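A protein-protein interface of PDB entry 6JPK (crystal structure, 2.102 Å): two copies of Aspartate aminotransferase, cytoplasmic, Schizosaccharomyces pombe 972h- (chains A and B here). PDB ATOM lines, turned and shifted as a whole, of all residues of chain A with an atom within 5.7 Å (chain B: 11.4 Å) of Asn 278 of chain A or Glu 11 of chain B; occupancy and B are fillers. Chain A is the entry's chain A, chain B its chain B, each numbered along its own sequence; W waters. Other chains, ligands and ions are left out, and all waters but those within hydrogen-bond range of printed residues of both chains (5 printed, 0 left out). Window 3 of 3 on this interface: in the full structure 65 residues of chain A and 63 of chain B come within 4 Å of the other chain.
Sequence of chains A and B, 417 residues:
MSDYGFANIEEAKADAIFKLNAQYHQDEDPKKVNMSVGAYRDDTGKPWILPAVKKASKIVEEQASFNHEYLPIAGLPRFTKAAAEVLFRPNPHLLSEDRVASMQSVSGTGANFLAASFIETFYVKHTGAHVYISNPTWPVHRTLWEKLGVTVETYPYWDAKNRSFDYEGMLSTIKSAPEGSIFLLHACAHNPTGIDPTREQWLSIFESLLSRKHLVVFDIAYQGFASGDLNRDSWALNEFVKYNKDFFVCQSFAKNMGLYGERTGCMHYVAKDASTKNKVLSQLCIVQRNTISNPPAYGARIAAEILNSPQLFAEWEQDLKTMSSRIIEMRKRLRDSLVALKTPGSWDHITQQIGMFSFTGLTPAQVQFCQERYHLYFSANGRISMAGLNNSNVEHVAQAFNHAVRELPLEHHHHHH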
ATOM      1  N   ASP A  98      28.593  21.476   6.828  1.00  0.00           N
ATOM      2  CA  ASP A  98      27.716  21.145   5.697  1.00  0.00           C
ATOM      3  C   ASP A  98      26.247  21.109   6.129  1.00  0.00           C
ATOM      4  O   ASP A  98      25.479  20.233   5.720  1.00  0.00           O
ATOM      5  CB  ASP A  98      28.133  19.811   5.054  1.00  0.00           C
ATOM      6  CG  ASP A  98      27.503  19.583   3.683  1.00  0.00           C
ATOM      7  OD1 ASP A  98      27.393  20.552   2.902  1.00  0.00           O
ATOM      8  OD2 ASP A  98      27.137  18.422   3.383  1.00  0.00           O
ATOM      9  N   ASP A 273      21.620  18.861  10.784  1.00  0.00           N
ATOM     10  CA  ASP A 273      22.674  17.935  10.387  1.00  0.00           C
ATOM     11  C   ASP A 273      22.739  17.858   8.867  1.00  0.00           C
ATOM     12  O   ASP A 273      21.786  18.215   8.162  1.00  0.00           O
ATOM     13  CB  ASP A 273      22.461  16.547  10.993  1.00  0.00           C
ATOM     14  CG  ASP A 273      21.084  16.010  10.727  1.00  0.00           C
ATOM     15  OD1 ASP A 273      20.791  15.733   9.541  1.00  0.00           O
ATOM     16  OD2 ASP A 273      20.296  15.872  11.703  1.00  0.00           O
ATOM     17  N   ALA A 274      23.883  17.370   8.383  1.00  0.00           N
ATOM     18  CA  ALA A 274      24.147  17.329   6.948  1.00  0.00           C
ATOM     19  C   ALA A 274      23.151  16.432   6.227  1.00  0.00           C
ATOM     20  O   ALA A 274      22.755  16.720   5.092  1.00  0.00           O
ATOM     21  CB  ALA A 274      25.581  16.842   6.695  1.00  0.00           C
ATOM     22  N   SER A 275      22.757  15.330   6.866  1.00  0.00           N
ATOM     23  CA  SER A 275      21.801  14.405   6.267  1.00  0.00           C
ATOM     24  C   SER A 275      20.503  15.113   5.881  1.00  0.00           C
ATOM     25  O   SER A 275      20.030  14.997   4.744  1.00  0.00           O
ATOM     26  CB  SER A 275      21.520  13.260   7.239  1.00  0.00           C
ATOM     27  OG  SER A 275      20.585  12.370   6.667  1.00  0.00           O
ATOM     28  N   THR A 276      19.913  15.860   6.813  1.00  0.00           N
ATOM     29  CA  THR A 276      18.668  16.563   6.497  1.00  0.00           C
ATOM     30  C   THR A 276      18.909  17.724   5.530  1.00  0.00           C
ATOM     31  O   THR A 276      18.063  18.003   4.667  1.00  0.00           O
ATOM     32  CB  THR A 276      18.019  17.052   7.791  1.00  0.00           C
ATOM     33  OG1 THR A 276      17.793  15.929   8.650  1.00  0.00           O
ATOM     34  CG2 THR A 276      16.688  17.795   7.523  1.00  0.00           C
ATOM     35  N   LYS A 277      20.060  18.393   5.647  1.00  0.00           N
ATOM     36  CA  LYS A 277      20.447  19.401   4.665  1.00  0.00           C
ATOM     37  C   LYS A 277      20.321  18.858   3.248  1.00  0.00           C
ATOM     38  O   LYS A 277      19.758  19.509   2.364  1.00  0.00           O
ATOM     39  CB  LYS A 277      21.880  19.868   4.943  1.00  0.00           C
ATOM     40  CG  LYS A 277      22.318  21.093   4.144  1.00  0.00           C
ATOM     41  CD  LYS A 277      22.822  20.764   2.750  1.00  0.00           C
ATOM     42  CE  LYS A 277      24.111  19.994   2.783  1.00  0.00           C
ATOM     43  NZ  LYS A 277      24.856  20.176   1.501  1.00  0.00           N
ATOM     44  N   ASN A 278      20.837  17.654   3.013  1.00  0.00           N
ATOM     45  CA  ASN A 278      20.816  17.116   1.658  1.00  0.00           C
ATOM     46  C   ASN A 278      19.427  16.646   1.241  1.00  0.00           C
ATOM     47  O   ASN A 278      19.062  16.790   0.071  1.00  0.00           O
ATOM     48  CB  ASN A 278      21.852  16.005   1.539  1.00  0.00           C
ATOM     49  CG  ASN A 278      23.260  16.566   1.512  1.00  0.00           C
ATOM     50  OD1 ASN A 278      23.525  17.548   0.813  1.00  0.00           O
ATOM     51  ND2 ASN A 278      24.150  15.994   2.309  1.00  0.00           N
ATOM     52  N   LYS A 279      18.630  16.107   2.164  1.00  0.00           N
ATOM     53  CA  LYS A 279      17.249  15.761   1.817  1.00  0.00           C
ATOM     54  C   LYS A 279      16.482  16.996   1.349  1.00  0.00           C
ATOM     55  O   LYS A 279      15.842  16.985   0.285  1.00  0.00           O
ATOM     56  CB  LYS A 279      16.556  15.113   3.018  1.00  0.00           C
ATOM     57  CG  LYS A 279      17.119  13.745   3.380  1.00  0.00           C
ATOM     58  CD  LYS A 279      16.627  13.274   4.743  1.00  0.00           C
ATOM     59  CE  LYS A 279      17.031  11.825   5.009  1.00  0.00           C
ATOM     60  NZ  LYS A 279      16.842  11.435   6.446  1.00  0.00           N
ATOM     61  N   VAL A 280      16.567  18.080   2.124  1.00  0.00           N
ATOM     62  CA  VAL A 280      15.856  19.311   1.803  1.00  0.00           C
ATOM     63  C   VAL A 280      16.389  19.908   0.504  1.00  0.00           C
ATOM     64  O   VAL A 280      15.619  20.325  -0.372  1.00  0.00           O
ATOM     65  CB  VAL A 280      15.971  20.301   2.982  1.00  0.00           C
ATOM     66  CG1 VAL A 280      15.526  21.711   2.585  1.00  0.00           C
ATOM     67  CG2 VAL A 280      15.190  19.791   4.178  1.00  0.00           C
ATOM     68  N   LEU A 281      17.719  19.967   0.365  1.00  0.00           N
ATOM     69  CA  LEU A 281      18.309  20.524  -0.852  1.00  0.00           C
ATOM     70  C   LEU A 281      17.796  19.804  -2.096  1.00  0.00           C
ATOM     71  O   LEU A 281      17.434  20.448  -3.083  1.00  0.00           O
ATOM     72  CB  LEU A 281      19.835  20.458  -0.783  1.00  0.00           C
ATOM     73  CG  LEU A 281      20.578  21.037  -1.989  1.00  0.00           C
ATOM     74  CD1 LEU A 281      20.293  22.523  -2.158  1.00  0.00           C
ATOM     75  CD2 LEU A 281      22.072  20.784  -1.834  1.00  0.00           C
ATOM     76  N   SER A 282      17.722  18.467  -2.056  1.00  0.00           N
ATOM     77  CA  SER A 282      17.265  17.720  -3.226  1.00  0.00           C
ATOM     78  C   SER A 282      15.835  18.097  -3.608  1.00  0.00           C
ATOM     79  O   SER A 282      15.496  18.163  -4.800  1.00  0.00           O
ATOM     80  CB  SER A 282      17.380  16.211  -2.971  1.00  0.00           C
ATOM     81  OG  SER A 282      16.424  15.752  -2.020  1.00  0.00           O
ATOM     82  N   GLN A 283      14.977  18.345  -2.610  1.00  0.00           N
ATOM     83  CA  GLN A 283      13.600  18.732  -2.896  1.00  0.00           C
ATOM     84  C   GLN A 283      13.496  20.172  -3.379  1.00  0.00           C
ATOM     85  O   GLN A 283      12.623  20.483  -4.202  1.00  0.00           O
ATOM     86  CB  GLN A 283      12.730  18.538  -1.653  1.00  0.00           C
ATOM     87  CG  GLN A 283      12.613  17.095  -1.232  1.00  0.00           C
ATOM     88  CD  GLN A 283      11.961  16.240  -2.300  1.00  0.00           C
ATOM     89  OE1 GLN A 283      11.239  16.748  -3.168  1.00  0.00           O
ATOM     90  NE2 GLN A 283      12.219  14.937  -2.249  1.00  0.00           N
ATOM     91  N   SER B   2      13.310  19.312  10.972  1.00  0.00           N
ATOM     92  CA  SER B   2      13.892  18.292  11.851  1.00  0.00           C
ATOM     93  C   SER B   2      13.458  18.407  13.302  1.00  0.00           C
ATOM     94  O   SER B   2      13.140  17.402  13.924  1.00  0.00           O
ATOM     95  CB  SER B   2      15.386  18.329  11.839  1.00  0.00           C
ATOM     96  OG  SER B   2      15.866  17.193  12.549  1.00  0.00           O
ATOM     97  N   GLY B   5      10.027  17.756  11.454  1.00  0.00           N
ATOM     98  CA  GLY B   5       9.747  16.592  10.638  1.00  0.00           C
ATOM     99  C   GLY B   5      10.522  16.482   9.339  1.00  0.00           C
ATOM    100  O   GLY B   5      10.290  15.530   8.584  1.00  0.00           O
ATOM    101  N   PHE B   6      11.454  17.400   9.053  1.00  0.00           N
ATOM    102  CA  PHE B   6      12.118  17.380   7.749  1.00  0.00           C
ATOM    103  C   PHE B   6      13.092  16.216   7.588  1.00  0.00           C
ATOM    104  O   PHE B   6      13.482  15.902   6.456  1.00  0.00           O
ATOM    105  CB  PHE B   6      12.826  18.714   7.507  1.00  0.00           C
ATOM    106  CG  PHE B   6      11.877  19.885   7.406  1.00  0.00           C
ATOM    107  CD1 PHE B   6      10.674  19.762   6.725  1.00  0.00           C
ATOM    108  CD2 PHE B   6      12.168  21.089   8.022  1.00  0.00           C
ATOM    109  CE1 PHE B   6       9.791  20.835   6.645  1.00  0.00           C
ATOM    110  CE2 PHE B   6      11.301  22.160   7.943  1.00  0.00           C
ATOM    111  CZ  PHE B   6      10.109  22.041   7.265  1.00  0.00           C
ATOM    112  N   ALA B   7      13.493  15.559   8.678  1.00  0.00           N
ATOM    113  CA  ALA B   7      14.331  14.370   8.552  1.00  0.00           C
ATOM    114  C   ALA B   7      13.577  13.194   7.957  1.00  0.00           C
ATOM    115  O   ALA B   7      14.216  12.245   7.486  1.00  0.00           O
ATOM    116  CB  ALA B   7      14.902  13.955   9.911  1.00  0.00           C
ATOM    117  N   ASN B   8      12.240  13.226   7.985  1.00  0.00           N
ATOM    118  CA  ASN B   8      11.418  12.179   7.386  1.00  0.00           C
ATOM    119  C   ASN B   8      11.285  12.313   5.877  1.00  0.00           C
ATOM    120  O   ASN B   8      10.683  11.442   5.244  1.00  0.00           O
ATOM    121  CB  ASN B   8      10.016  12.184   8.009  1.00  0.00           C
ATOM    122  CG  ASN B   8      10.051  11.987   9.506  1.00  0.00           C
ATOM    123  OD1 ASN B   8      10.958  11.339  10.033  1.00  0.00           O
ATOM    124  ND2 ASN B   8       9.068  12.553  10.206  1.00  0.00           N
ATOM    125  N   ILE B   9      11.821  13.377   5.283  1.00  0.00           N
ATOM    126  CA  ILE B   9      11.767  13.527   3.834  1.00  0.00           C
ATOM    127  C   ILE B   9      12.724  12.538   3.177  1.00  0.00           C
ATOM    128  O   ILE B   9      13.835  12.308   3.665  1.00  0.00           O
ATOM    129  CB  ILE B   9      12.106  14.981   3.463  1.00  0.00           C
ATOM    130  CG1 ILE B   9      10.978  15.911   3.910  1.00  0.00           C
ATOM    131  CG2 ILE B   9      12.391  15.120   1.989  1.00  0.00           C
ATOM    132  CD1 ILE B   9      11.329  17.382   3.741  1.00  0.00           C
ATOM    133  N   GLU B  10      12.291  11.924   2.077  1.00  0.00           N
ATOM    134  CA  GLU B  10      13.182  11.107   1.265  1.00  0.00           C
ATOM    135  C   GLU B  10      13.909  11.981   0.248  1.00  0.00           C
ATOM    136  O   GLU B  10      13.292  12.809  -0.434  1.00  0.00           O
ATOM    137  CB  GLU B  10      12.414   9.991   0.558  1.00  0.00           C
ATOM    138  CG  GLU B  10      12.174   8.775   1.439  1.00  0.00           C
ATOM    139  CD  GLU B  10      11.406   7.674   0.733  1.00  0.00           C
ATOM    140  OE1 GLU B  10      10.956   7.902  -0.409  1.00  0.00           O
ATOM    141  OE2 GLU B  10      11.249   6.583   1.324  1.00  0.00           O
ATOM    142  N   GLU B  11      15.224  11.809   0.178  1.00  0.00           N
ATOM    143  CA  GLU B  11      16.033  12.565  -0.762  1.00  0.00           C
ATOM    144  C   GLU B  11      15.637  12.195  -2.185  1.00  0.00           C
ATOM    145  O   GLU B  11      15.526  11.013  -2.521  1.00  0.00           O
ATOM    146  CB  GLU B  11      17.514  12.276  -0.514  1.00  0.00           C
ATOM    147  CG  GLU B  11      18.469  13.163  -1.292  1.00  0.00           C
ATOM    148  CD  GLU B  11      19.921  12.977  -0.872  1.00  0.00           C
ATOM    149  OE1 GLU B  11      20.807  13.601  -1.496  1.00  0.00           O
ATOM    150  OE2 GLU B  11      20.181  12.207   0.077  1.00  0.00           O
ATOM    151  N   ALA B  12      15.386  13.207  -3.012  1.00  0.00           N
ATOM    152  CA  ALA B  12      15.052  12.947  -4.405  1.00  0.00           C
ATOM    153  C   ALA B  12      16.250  12.337  -5.135  1.00  0.00           C
ATOM    154  O   ALA B  12      17.409  12.629  -4.827  1.00  0.00           O
ATOM    155  CB  ALA B  12      14.614  14.235  -5.091  1.00  0.00           C
ATOM    156  N   LYS B  13      15.968  11.469  -6.104  1.00  0.00           N
ATOM    157  CA  LYS B  13      17.067  10.867  -6.846  1.00  0.00           C
ATOM    158  C   LYS B  13      17.555  11.823  -7.929  1.00  0.00           C
ATOM    159  O   LYS B  13      16.822  12.695  -8.402  1.00  0.00           O
ATOM    160  CB  LYS B  13      16.654   9.529  -7.462  1.00  0.00           C
ATOM    161  N   ALA B  14      18.817  11.648  -8.315  1.00  0.00           N
ATOM    162  CA  ALA B  14      19.472  12.579  -9.222  1.00  0.00           C
ATOM    163  C   ALA B  14      18.822  12.567 -10.601  1.00  0.00           C
ATOM    164  O   ALA B  14      18.284  11.551 -11.049  1.00  0.00           O
ATOM    165  CB  ALA B  14      20.957  12.239  -9.355  1.00  0.00           C
ATOM    166  N   ASP B  15      18.867  13.721 -11.268  1.00  0.00           N
ATOM    167  CA  ASP B  15      18.463  13.794 -12.666  1.00  0.00           C
ATOM    168  C   ASP B  15      19.369  12.898 -13.503  1.00  0.00           C
ATOM    169  O   ASP B  15      20.563  12.762 -13.222  1.00  0.00           O
ATOM    170  CB  ASP B  15      18.524  15.241 -13.172  1.00  0.00           C
ATOM    171  N   PHE B  18      22.331  14.834 -15.161  1.00  0.00           N
ATOM    172  CA  PHE B  18      23.391  15.146 -14.205  1.00  0.00           C
ATOM    173  C   PHE B  18      24.248  13.919 -13.910  1.00  0.00           C
ATOM    174  O   PHE B  18      25.481  13.993 -13.921  1.00  0.00           O
ATOM    175  CB  PHE B  18      22.797  15.712 -12.910  1.00  0.00           C
ATOM    176  CG  PHE B  18      23.837  16.072 -11.874  1.00  0.00           C
ATOM    177  CD1 PHE B  18      24.352  17.365 -11.810  1.00  0.00           C
ATOM    178  CD2 PHE B  18      24.312  15.119 -10.978  1.00  0.00           C
ATOM    179  CE1 PHE B  18      25.313  17.704 -10.866  1.00  0.00           C
ATOM    180  CE2 PHE B  18      25.276  15.445 -10.029  1.00  0.00           C
ATOM    181  CZ  PHE B  18      25.778  16.741  -9.973  1.00  0.00           C
HETATM  182  O   HOH W   1      14.122  10.020   5.205  1.00  0.00           O
HETATM  183  O   HOH W   2      21.137  16.917  -2.245  1.00  0.00           O
HETATM  184  O   HOH W   3      15.727   9.648   8.919  1.00  0.00           O
HETATM  185  O   HOH W   4      17.762  17.076  10.965  1.00  0.00           O
HETATM  186  O   HOH W   5      20.605  12.800   3.170  1.00  0.00           O
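The side-chain amino group (NZ) of Lys 279 of chain A lies within hydrogen-bond range of the backbone carbonyl oxygen (O) of Ala 7 of chain B, at 2.9 Å.
The side-chain hydroxyl (OG) of Ser 282 of chain A sits at hydrogen-bond distance from the backbone NH (N) of Ala 12 of chain B (2.9 Å).
The side-chain amide nitrogen (NE2) of Gln 283 of chain A is in hydrogen-bond range of the backbone carbonyl oxygen (O) of Glu 10 of chain B, at 3.0 Å.
The side-chain carboxylate (OD1) of Asp 273 of chain A is in hydrogen-bond range of the backbone NH (N) of Thr 276 of chain A.
The backbone carbonyl oxygen (O) of Ala 274 of chain A is in hydrogen-bond range of the side-chain amide nitrogen (ND2) of Asn 278 of chain A (3.2 Å).
OD1 of Asn 278 of chain A is in hydrogen-bond range of NZ of Lys 277 of chain A, at 3.0 Å.
The backbone carbonyl oxygen of Lys 279 of chain A sits at hydrogen-bond distance from the side-chain hydroxyl of Ser 282 of chain A.
CG2 of Thr 276 of chain A touches O of Phe 6 of chain B, at 3.9 Å.
CB of Ala 7 of chain B touches OG1 of Thr 276 of chain A, 3.7 Å away.
Asn 278 of chain A touches Glu 11 of chain B.
CD of Lys 279 of chain A touches O of Ile 9 of chain B, 3.1 Å away.
Ser 282 of chain A touches Glu 11 of chain B (OG to CG, 3.4 Å).
CG2 of Ile 9 of chain B touches CG of Gln 283 of chain A (3.8 Å).
N of Ala 12 of chain B touches NE2 of Gln 283 of chain A, at 3.7 Å.
No residue of chain B comes within 4 Å of Ala 274 of chain A.
No residue of chain B comes within 4 Å of Ser 275 of chain A.
Thr 276 of chain A touches two residues of chain B.
No residue of chain B comes within 4 Å of Lys 277 of chain A.
Of chain B, only Glu 11 comes within 4 Å of Asn 278 of chain A.
Of chain B, only Ala 7 and Ile 9 come within 4 Å of Lys 279 of chain A.
No residue of chain B comes within 4 Å of Leu 281 of chain A.
Of the printed residues of chain B, Gln 283 of chain A touches Ile 9 (3.8 Å), Glu 10 (3.0 Å) and Ala 12 (3.7 Å).
Of the printed residues of chain A, Ala 7 of chain B touches Thr 276 and Lys 279.
Of the printed residues of chain A, Glu 10 of chain B touches Gln 283 (3.0 Å).
Of chain A, only Asn 278 (3.9 Å) and Ser 282 (3.4 Å) come within 4 Å of Glu 11 of chain B.
The nearest residue of chain B that does not touch Asn 278 of chain A is Ala 12 of chain B (6.0 Å).
The nearest residue of chain A that does not touch Glu 11 of chain B is Lys 279 of chain A (4.2 Å).
Of the 13 printed residues of chain B, 6 touch a printed residue of chain A.
Printed residues of chain B that touch a printed residue of chain A: Phe 6, Ala 7, Ile 9, Glu 10, Glu 11 and Ala 12.
Hydrophobic or aromatic side chains of chain B that line the printed part of chain A: Phe 6, Ala 7, Ile 9 and Ala 12.
No position is printed for both chains.
Of the 10 pairs that touch across the chains among the printed residues, none has its exchanged pair printed and touching as well.
Water W4 lies within hydrogen-bond range of the side-chain hydroxyl (OG) of Ser 2 of chain B, the side-chain hydroxyl (OG1) of Thr 276 of chain A and the side-chain carboxylate (OD2) of Asp 273 of chain A.
Water W5 bridges O of Ser 275 of chain A and OE2 of Glu 11 of chain B.
Water W1 lies within hydrogen-bond range of the backbone carbonyl oxygen of Ile 9 of chain B (2.8 Å), the backbone carbonyl oxygen of Ala 7 of chain B (3.2 Å) and the side-chain amino group of Lys 279 of chain A (3.3 Å).
Water W2 bridges O of Asn 278 of chain A (3.1 Å) and OE1 of Glu 11 of chain B (3.4 Å).
Water W3 lies within hydrogen-bond range of NZ of Lys 279 of chain A and O of Ala 7 of chain B.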
